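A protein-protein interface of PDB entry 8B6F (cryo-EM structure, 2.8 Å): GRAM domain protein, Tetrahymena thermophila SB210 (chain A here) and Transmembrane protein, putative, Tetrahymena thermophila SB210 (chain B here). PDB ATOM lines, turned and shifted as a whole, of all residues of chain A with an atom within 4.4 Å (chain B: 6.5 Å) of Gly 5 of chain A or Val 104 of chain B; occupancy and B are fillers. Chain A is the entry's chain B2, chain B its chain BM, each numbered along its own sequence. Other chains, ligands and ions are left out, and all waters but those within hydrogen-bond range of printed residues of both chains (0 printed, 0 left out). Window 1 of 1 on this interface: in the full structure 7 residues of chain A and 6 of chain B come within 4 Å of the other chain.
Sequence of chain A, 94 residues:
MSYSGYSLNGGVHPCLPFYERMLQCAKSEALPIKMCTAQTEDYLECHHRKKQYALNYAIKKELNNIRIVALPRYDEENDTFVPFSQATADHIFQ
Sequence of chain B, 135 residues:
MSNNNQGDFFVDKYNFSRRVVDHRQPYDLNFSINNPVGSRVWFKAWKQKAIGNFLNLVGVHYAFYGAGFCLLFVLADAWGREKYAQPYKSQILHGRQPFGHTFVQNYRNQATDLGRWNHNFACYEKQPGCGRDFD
The backbone carbonyl oxygen of Gly 5 of chain A is in hydrogen-bond range of the backbone NH of His 13 of chain A (2.8 Å). The backbone carbonyl oxygen (O) of Phe 103 of chain B lies within hydrogen-bond range of the side-chain hydroxyl (OH) of Tyr 124 of chain B (3.0 Å).
Among the printed residues, pairs that only touch across the chains: Ser 4 of chain A with Val 104 of chain B (3.6 Å), Gly 5 of chain A with Val 104 of chain B (3.9 Å), Tyr 6 of chain A with Gly 100 of chain B (3.4 Å), Tyr 6 of chain A with His 101 of chain B (3.9 Å), Tyr 6 of chain A with Val 104 of chain B (3.5 Å), Tyr 6 of chain A with Gln 105 of chain B (3.9 Å) and Val 12 of chain A with Phe 103 of chain B (3.3 Å).
Tyr 3 of chain A touches none of the printed residues of chain B. Printed residues of chain B within 4 Å of Ser 4 of chain A: Val 104. Of the printed residues of chain B, Gly 5 of chain A touches Val 104 (3.9 Å). Printed residues of chain B within 4 Å of Val 12 of chain A: Phe 103 (3.3 Å). Printed residues of chain A within 4 Å of Phe 103 of chain B: Val 12. The nearest residue of chain A that does not touch Val 104 of chain B is Val 12 of chain A (4.2 Å).
Hydrophobic or aromatic side chains of chain B within 4 Å of the printed part of chain A: Phe 103 and Val 104. Along chain B the printed residues that touch a printed residue of chain A span positions 100 to 105. Among the printed residues, no Asp or Glu carboxylate lies within 4 Å of a Lys or Arg side-chain nitrogen of the other chain.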
ATOM      1  N   TYR A   3     -10.428 -24.301 -38.200  1.00  0.00           N
ATOM      2  CA  TYR A   3     -11.147 -25.070 -37.187  1.00  0.00           C
ATOM      3  C   TYR A   3     -12.133 -24.131 -36.502  1.00  0.00           C
ATOM      4  O   TYR A   3     -11.779 -23.415 -35.563  1.00  0.00           O
ATOM      5  CB  TYR A   3     -10.178 -25.688 -36.185  1.00  0.00           C
ATOM      6  CG  TYR A   3     -10.863 -26.497 -35.112  1.00  0.00           C
ATOM      7  CD1 TYR A   3     -11.202 -27.823 -35.333  1.00  0.00           C
ATOM      8  CD2 TYR A   3     -11.172 -25.934 -33.882  1.00  0.00           C
ATOM      9  CE1 TYR A   3     -11.829 -28.570 -34.360  1.00  0.00           C
ATOM     10  CE2 TYR A   3     -11.802 -26.674 -32.901  1.00  0.00           C
ATOM     11  CZ  TYR A   3     -12.130 -27.990 -33.151  1.00  0.00           C
ATOM     12  OH  TYR A   3     -12.753 -28.736 -32.185  1.00  0.00           O
ATOM     13  N   SER A   4     -13.376 -24.129 -36.981  1.00  0.00           N
ATOM     14  CA  SER A   4     -14.384 -23.232 -36.425  1.00  0.00           C
ATOM     15  C   SER A   4     -14.686 -23.564 -34.970  1.00  0.00           C
ATOM     16  O   SER A   4     -14.884 -22.662 -34.148  1.00  0.00           O
ATOM     17  CB  SER A   4     -15.657 -23.304 -37.260  1.00  0.00           C
ATOM     18  OG  SER A   4     -16.179 -24.614 -37.225  1.00  0.00           O
ATOM     19  N   GLY A   5     -14.732 -24.848 -34.633  1.00  0.00           N
ATOM     20  CA  GLY A   5     -15.054 -25.267 -33.286  1.00  0.00           C
ATOM     21  C   GLY A   5     -16.530 -25.383 -32.981  1.00  0.00           C
ATOM     22  O   GLY A   5     -16.891 -25.502 -31.804  1.00  0.00           O
ATOM     23  N   TYR A   6     -17.393 -25.351 -33.990  1.00  0.00           N
ATOM     24  CA  TYR A   6     -18.828 -25.503 -33.807  1.00  0.00           C
ATOM     25  C   TYR A   6     -19.266 -26.922 -34.151  1.00  0.00           C
ATOM     26  O   TYR A   6     -18.586 -27.653 -34.874  1.00  0.00           O
ATOM     27  CB  TYR A   6     -19.595 -24.508 -34.680  1.00  0.00           C
ATOM     28  CG  TYR A   6     -19.412 -23.065 -34.287  1.00  0.00           C
ATOM     29  CD1 TYR A   6     -20.122 -22.519 -33.227  1.00  0.00           C
ATOM     30  CD2 TYR A   6     -18.544 -22.241 -34.987  1.00  0.00           C
ATOM     31  CE1 TYR A   6     -19.963 -21.196 -32.869  1.00  0.00           C
ATOM     32  CE2 TYR A   6     -18.378 -20.918 -34.638  1.00  0.00           C
ATOM     33  CZ  TYR A   6     -19.090 -20.401 -33.578  1.00  0.00           C
ATOM     34  OH  TYR A   6     -18.927 -19.082 -33.229  1.00  0.00           O
ATOM     35  N   SER A   7     -20.423 -27.304 -33.618  1.00  0.00           N
ATOM     36  CA  SER A   7     -21.030 -28.586 -33.933  1.00  0.00           C
ATOM     37  C   SER A   7     -22.002 -28.404 -35.097  1.00  0.00           C
ATOM     38  O   SER A   7     -22.067 -27.339 -35.716  1.00  0.00           O
ATOM     39  CB  SER A   7     -21.714 -29.170 -32.699  1.00  0.00           C
ATOM     40  OG  SER A   7     -22.786 -28.350 -32.271  1.00  0.00           O
ATOM     41  N   GLY A  11     -23.645 -25.925 -31.640  1.00  0.00           N
ATOM     42  CA  GLY A  11     -22.985 -26.150 -30.369  1.00  0.00           C
ATOM     43  C   GLY A  11     -21.480 -26.059 -30.487  1.00  0.00           C
ATOM     44  O   GLY A  11     -20.939 -25.300 -31.298  1.00  0.00           O
ATOM     45  N   VAL A  12     -20.789 -26.846 -29.668  1.00  0.00           N
ATOM     46  CA  VAL A  12     -19.332 -26.862 -29.622  1.00  0.00           C
ATOM     47  C   VAL A  12     -18.836 -28.174 -30.209  1.00  0.00           C
ATOM     48  O   VAL A  12     -19.363 -29.247 -29.892  1.00  0.00           O
ATOM     49  CB  VAL A  12     -18.811 -26.657 -28.189  1.00  0.00           C
ATOM     50  CG1 VAL A  12     -17.364 -27.115 -28.053  1.00  0.00           C
ATOM     51  CG2 VAL A  12     -18.924 -25.197 -27.810  1.00  0.00           C
ATOM     52  N   HIS A  13     -17.823 -28.080 -31.063  1.00  0.00           N
ATOM     53  CA  HIS A  13     -17.258 -29.262 -31.687  1.00  0.00           C
ATOM     54  C   HIS A  13     -16.699 -30.190 -30.611  1.00  0.00           C
ATOM     55  O   HIS A  13     -16.041 -29.725 -29.674  1.00  0.00           O
ATOM     56  CB  HIS A  13     -16.154 -28.856 -32.666  1.00  0.00           C
ATOM     57  CG  HIS A  13     -15.769 -29.935 -33.626  1.00  0.00           C
ATOM     58  ND1 HIS A  13     -14.636 -30.703 -33.465  1.00  0.00           N
ATOM     59  CD2 HIS A  13     -16.361 -30.374 -34.760  1.00  0.00           C
ATOM     60  CE1 HIS A  13     -14.549 -31.571 -34.456  1.00  0.00           C
ATOM     61  NE2 HIS A  13     -15.583 -31.392 -35.257  1.00  0.00           N
ATOM     62  N   PHE B  99     -26.018 -19.529 -26.927  1.00  0.00           N
ATOM     63  CA  PHE B  99     -24.870 -19.958 -26.136  1.00  0.00           C
ATOM     64  C   PHE B  99     -23.783 -20.557 -27.019  1.00  0.00           C
ATOM     65  O   PHE B  99     -22.590 -20.339 -26.782  1.00  0.00           O
ATOM     66  CB  PHE B  99     -25.303 -20.960 -25.067  1.00  0.00           C
ATOM     67  CG  PHE B  99     -25.646 -22.314 -25.608  1.00  0.00           C
ATOM     68  CD1 PHE B  99     -26.900 -22.568 -26.133  1.00  0.00           C
ATOM     69  CD2 PHE B  99     -24.713 -23.338 -25.587  1.00  0.00           C
ATOM     70  CE1 PHE B  99     -27.216 -23.815 -26.631  1.00  0.00           C
ATOM     71  CE2 PHE B  99     -25.022 -24.587 -26.083  1.00  0.00           C
ATOM     72  CZ  PHE B  99     -26.276 -24.826 -26.605  1.00  0.00           C
ATOM     73  N   GLY B 100     -24.172 -21.321 -28.038  1.00  0.00           N
ATOM     74  CA  GLY B 100     -23.183 -21.872 -28.947  1.00  0.00           C
ATOM     75  C   GLY B 100     -22.352 -20.791 -29.611  1.00  0.00           C
ATOM     76  O   GLY B 100     -21.132 -20.916 -29.728  1.00  0.00           O
ATOM     77  N   HIS B 101     -23.003 -19.714 -30.052  1.00  0.00           N
ATOM     78  CA  HIS B 101     -22.273 -18.583 -30.611  1.00  0.00           C
ATOM     79  C   HIS B 101     -21.366 -17.949 -29.565  1.00  0.00           C
ATOM     80  O   HIS B 101     -20.163 -17.779 -29.786  1.00  0.00           O
ATOM     81  CB  HIS B 101     -23.253 -17.540 -31.152  1.00  0.00           C
ATOM     82  CG  HIS B 101     -24.044 -18.000 -32.339  1.00  0.00           C
ATOM     83  ND1 HIS B 101     -24.185 -17.236 -33.478  1.00  0.00           N
ATOM     84  CD2 HIS B 101     -24.742 -19.138 -32.561  1.00  0.00           C
ATOM     85  CE1 HIS B 101     -24.934 -17.885 -34.350  1.00  0.00           C
ATOM     86  NE2 HIS B 101     -25.285 -19.043 -33.819  1.00  0.00           N
ATOM     87  N   THR B 102     -21.927 -17.605 -28.405  1.00  0.00           N
ATOM     88  CA  THR B 102     -21.196 -16.770 -27.458  1.00  0.00           C
ATOM     89  C   THR B 102     -19.980 -17.496 -26.893  1.00  0.00           C
ATOM     90  O   THR B 102     -18.927 -16.882 -26.693  1.00  0.00           O
ATOM     91  CB  THR B 102     -22.129 -16.304 -26.335  1.00  0.00           C
ATOM     92  OG1 THR B 102     -21.529 -15.206 -25.639  1.00  0.00           O
ATOM     93  CG2 THR B 102     -22.389 -17.413 -25.334  1.00  0.00           C
ATOM     94  N   PHE B 103     -20.103 -18.796 -26.615  1.00  0.00           N
ATOM     95  CA  PHE B 103     -18.970 -19.525 -26.054  1.00  0.00           C
ATOM     96  C   PHE B 103     -17.778 -19.510 -27.000  1.00  0.00           C
ATOM     97  O   PHE B 103     -16.657 -19.178 -26.601  1.00  0.00           O
ATOM     98  CB  PHE B 103     -19.361 -20.967 -25.736  1.00  0.00           C
ATOM     99  CG  PHE B 103     -18.202 -21.810 -25.298  1.00  0.00           C
ATOM    100  CD1 PHE B 103     -17.760 -21.773 -23.988  1.00  0.00           C
ATOM    101  CD2 PHE B 103     -17.538 -22.621 -26.201  1.00  0.00           C
ATOM    102  CE1 PHE B 103     -16.687 -22.535 -23.582  1.00  0.00           C
ATOM    103  CE2 PHE B 103     -16.462 -23.386 -25.803  1.00  0.00           C
ATOM    104  CZ  PHE B 103     -16.036 -23.344 -24.491  1.00  0.00           C
ATOM    105  N   VAL B 104     -18.001 -19.867 -28.264  1.00  0.00           N
ATOM    106  CA  VAL B 104     -16.904 -19.906 -29.222  1.00  0.00           C
ATOM    107  C   VAL B 104     -16.364 -18.505 -29.470  1.00  0.00           C
ATOM    108  O   VAL B 104     -15.158 -18.315 -29.668  1.00  0.00           O
ATOM    109  CB  VAL B 104     -17.362 -20.577 -30.529  1.00  0.00           C
ATOM    110  CG1 VAL B 104     -16.238 -20.580 -31.557  1.00  0.00           C
ATOM    111  CG2 VAL B 104     -17.837 -21.995 -30.256  1.00  0.00           C
ATOM    112  N   GLN B 105     -17.242 -17.503 -29.461  1.00  0.00           N
ATOM    113  CA  GLN B 105     -16.803 -16.141 -29.737  1.00  0.00           C
ATOM    114  C   GLN B 105     -15.941 -15.581 -28.614  1.00  0.00           C
ATOM    115  O   GLN B 105     -15.022 -14.799 -28.878  1.00  0.00           O
ATOM    116  CB  GLN B 105     -18.021 -15.251 -29.973  1.00  0.00           C
ATOM    117  CG  GLN B 105     -18.810 -15.603 -31.224  1.00  0.00           C
ATOM    118  CD  GLN B 105     -18.119 -15.164 -32.489  1.00  0.00           C
ATOM    119  OE1 GLN B 105     -16.962 -14.749 -32.466  1.00  0.00           O
ATOM    120  NE2 GLN B 105     -18.836 -15.229 -33.606  1.00  0.00           N
ATOM    121  N   ASN B 106     -16.214 -15.958 -27.364  1.00  0.00           N
ATOM    122  CA  ASN B 106     -15.563 -15.354 -26.209  1.00  0.00           C
ATOM    123  C   ASN B 106     -14.853 -16.387 -25.340  1.00  0.00           C
ATOM    124  O   ASN B 106     -14.681 -16.173 -24.140  1.00  0.00           O
ATOM    125  CB  ASN B 106     -16.582 -14.586 -25.368  1.00  0.00           C
ATOM    126  CG  ASN B 106     -17.376 -13.589 -26.181  1.00  0.00           C
ATOM    127  OD1 ASN B 106     -16.840 -12.921 -27.060  1.00  0.00           O
ATOM    128  ND2 ASN B 106     -18.665 -13.486 -25.891  1.00  0.00           N
ATOM    129  N   TYR B 107     -14.427 -17.511 -25.921  1.00  0.00           N
ATOM    130  CA  TYR B 107     -13.794 -18.554 -25.116  1.00  0.00           C
ATOM    131  C   TYR B 107     -12.512 -18.045 -24.467  1.00  0.00           C
ATOM    132  O   TYR B 107     -12.415 -17.947 -23.239  1.00  0.00           O
ATOM    133  CB  TYR B 107     -13.511 -19.783 -25.982  1.00  0.00           C
ATOM    134  CG  TYR B 107     -12.996 -20.986 -25.213  1.00  0.00           C
ATOM    135  CD1 TYR B 107     -13.108 -21.061 -23.828  1.00  0.00           C
ATOM    136  CD2 TYR B 107     -12.390 -22.042 -25.877  1.00  0.00           C
ATOM    137  CE1 TYR B 107     -12.636 -22.155 -23.132  1.00  0.00           C
ATOM    138  CE2 TYR B 107     -11.915 -23.142 -25.188  1.00  0.00           C
ATOM    139  CZ  TYR B 107     -12.040 -23.192 -23.815  1.00  0.00           C
ATOM    140  OH  TYR B 107     -11.569 -24.282 -23.124  1.00  0.00           O
ATOM    141  N   ARG B 108     -11.514 -17.713 -25.284  1.00  0.00           N
ATOM    142  CA  ARG B 108     -10.247 -17.169 -24.813  1.00  0.00           C
ATOM    143  C   ARG B 108     -10.087 -15.711 -25.224  1.00  0.00           C
ATOM    144  O   ARG B 108      -8.979 -15.256 -25.518  1.00  0.00           O
ATOM    145  CB  ARG B 108      -9.078 -18.000 -25.340  1.00  0.00           C
ATOM    146  CG  ARG B 108      -9.099 -19.456 -24.906  1.00  0.00           C
ATOM    147  CD  ARG B 108      -9.046 -19.587 -23.394  1.00  0.00           C
ATOM    148  NE  ARG B 108      -8.838 -20.966 -22.973  1.00  0.00           N
ATOM    149  CZ  ARG B 108      -8.808 -21.368 -21.710  1.00  0.00           C
ATOM    150  NH1 ARG B 108      -8.982 -20.520 -20.709  1.00  0.00           N
ATOM    151  NH2 ARG B 108      -8.595 -22.653 -21.443  1.00  0.00           N
ATOM    152  N   TRP B 117     -17.223 -20.776 -17.612  1.00  0.00           N
ATOM    153  CA  TRP B 117     -18.464 -21.101 -18.300  1.00  0.00           C
ATOM    154  C   TRP B 117     -19.337 -21.962 -17.397  1.00  0.00           C
ATOM    155  O   TRP B 117     -18.869 -22.961 -16.841  1.00  0.00           O
ATOM    156  CB  TRP B 117     -18.182 -21.833 -19.615  1.00  0.00           C
ATOM    157  CG  TRP B 117     -19.413 -22.217 -20.382  1.00  0.00           C
ATOM    158  CD1 TRP B 117     -20.070 -23.411 -20.330  1.00  0.00           C
ATOM    159  CD2 TRP B 117     -20.129 -21.406 -21.321  1.00  0.00           C
ATOM    160  NE1 TRP B 117     -21.151 -23.394 -21.177  1.00  0.00           N
ATOM    161  CE2 TRP B 117     -21.209 -22.174 -21.797  1.00  0.00           C
ATOM    162  CE3 TRP B 117     -19.961 -20.105 -21.804  1.00  0.00           C
ATOM    163  CZ2 TRP B 117     -22.118 -21.683 -22.731  1.00  0.00           C
ATOM    164  CZ3 TRP B 117     -20.864 -19.620 -22.733  1.00  0.00           C
ATOM    165  CH2 TRP B 117     -21.929 -20.407 -23.187  1.00  0.00           C
ATOM    166  N   TYR B 124     -21.473 -17.480 -19.285  1.00  0.00           N
ATOM    167  CA  TYR B 124     -20.282 -17.135 -18.531  1.00  0.00           C
ATOM    168  C   TYR B 124     -20.659 -16.514 -17.189  1.00  0.00           C
ATOM    169  O   TYR B 124     -21.789 -16.071 -16.973  1.00  0.00           O
ATOM    170  CB  TYR B 124     -19.404 -16.164 -19.319  1.00  0.00           C
ATOM    171  CG  TYR B 124     -18.695 -16.784 -20.500  1.00  0.00           C
ATOM    172  CD1 TYR B 124     -17.532 -17.521 -20.325  1.00  0.00           C
ATOM    173  CD2 TYR B 124     -19.180 -16.622 -21.790  1.00  0.00           C
ATOM    174  CE1 TYR B 124     -16.875 -18.082 -21.398  1.00  0.00           C
ATOM    175  CE2 TYR B 124     -18.529 -17.181 -22.870  1.00  0.00           C
ATOM    176  CZ  TYR B 124     -17.376 -17.909 -22.668  1.00  0.00           C
ATOM    177  OH  TYR B 124     -16.718 -18.470 -23.736  1.00  0.00           O
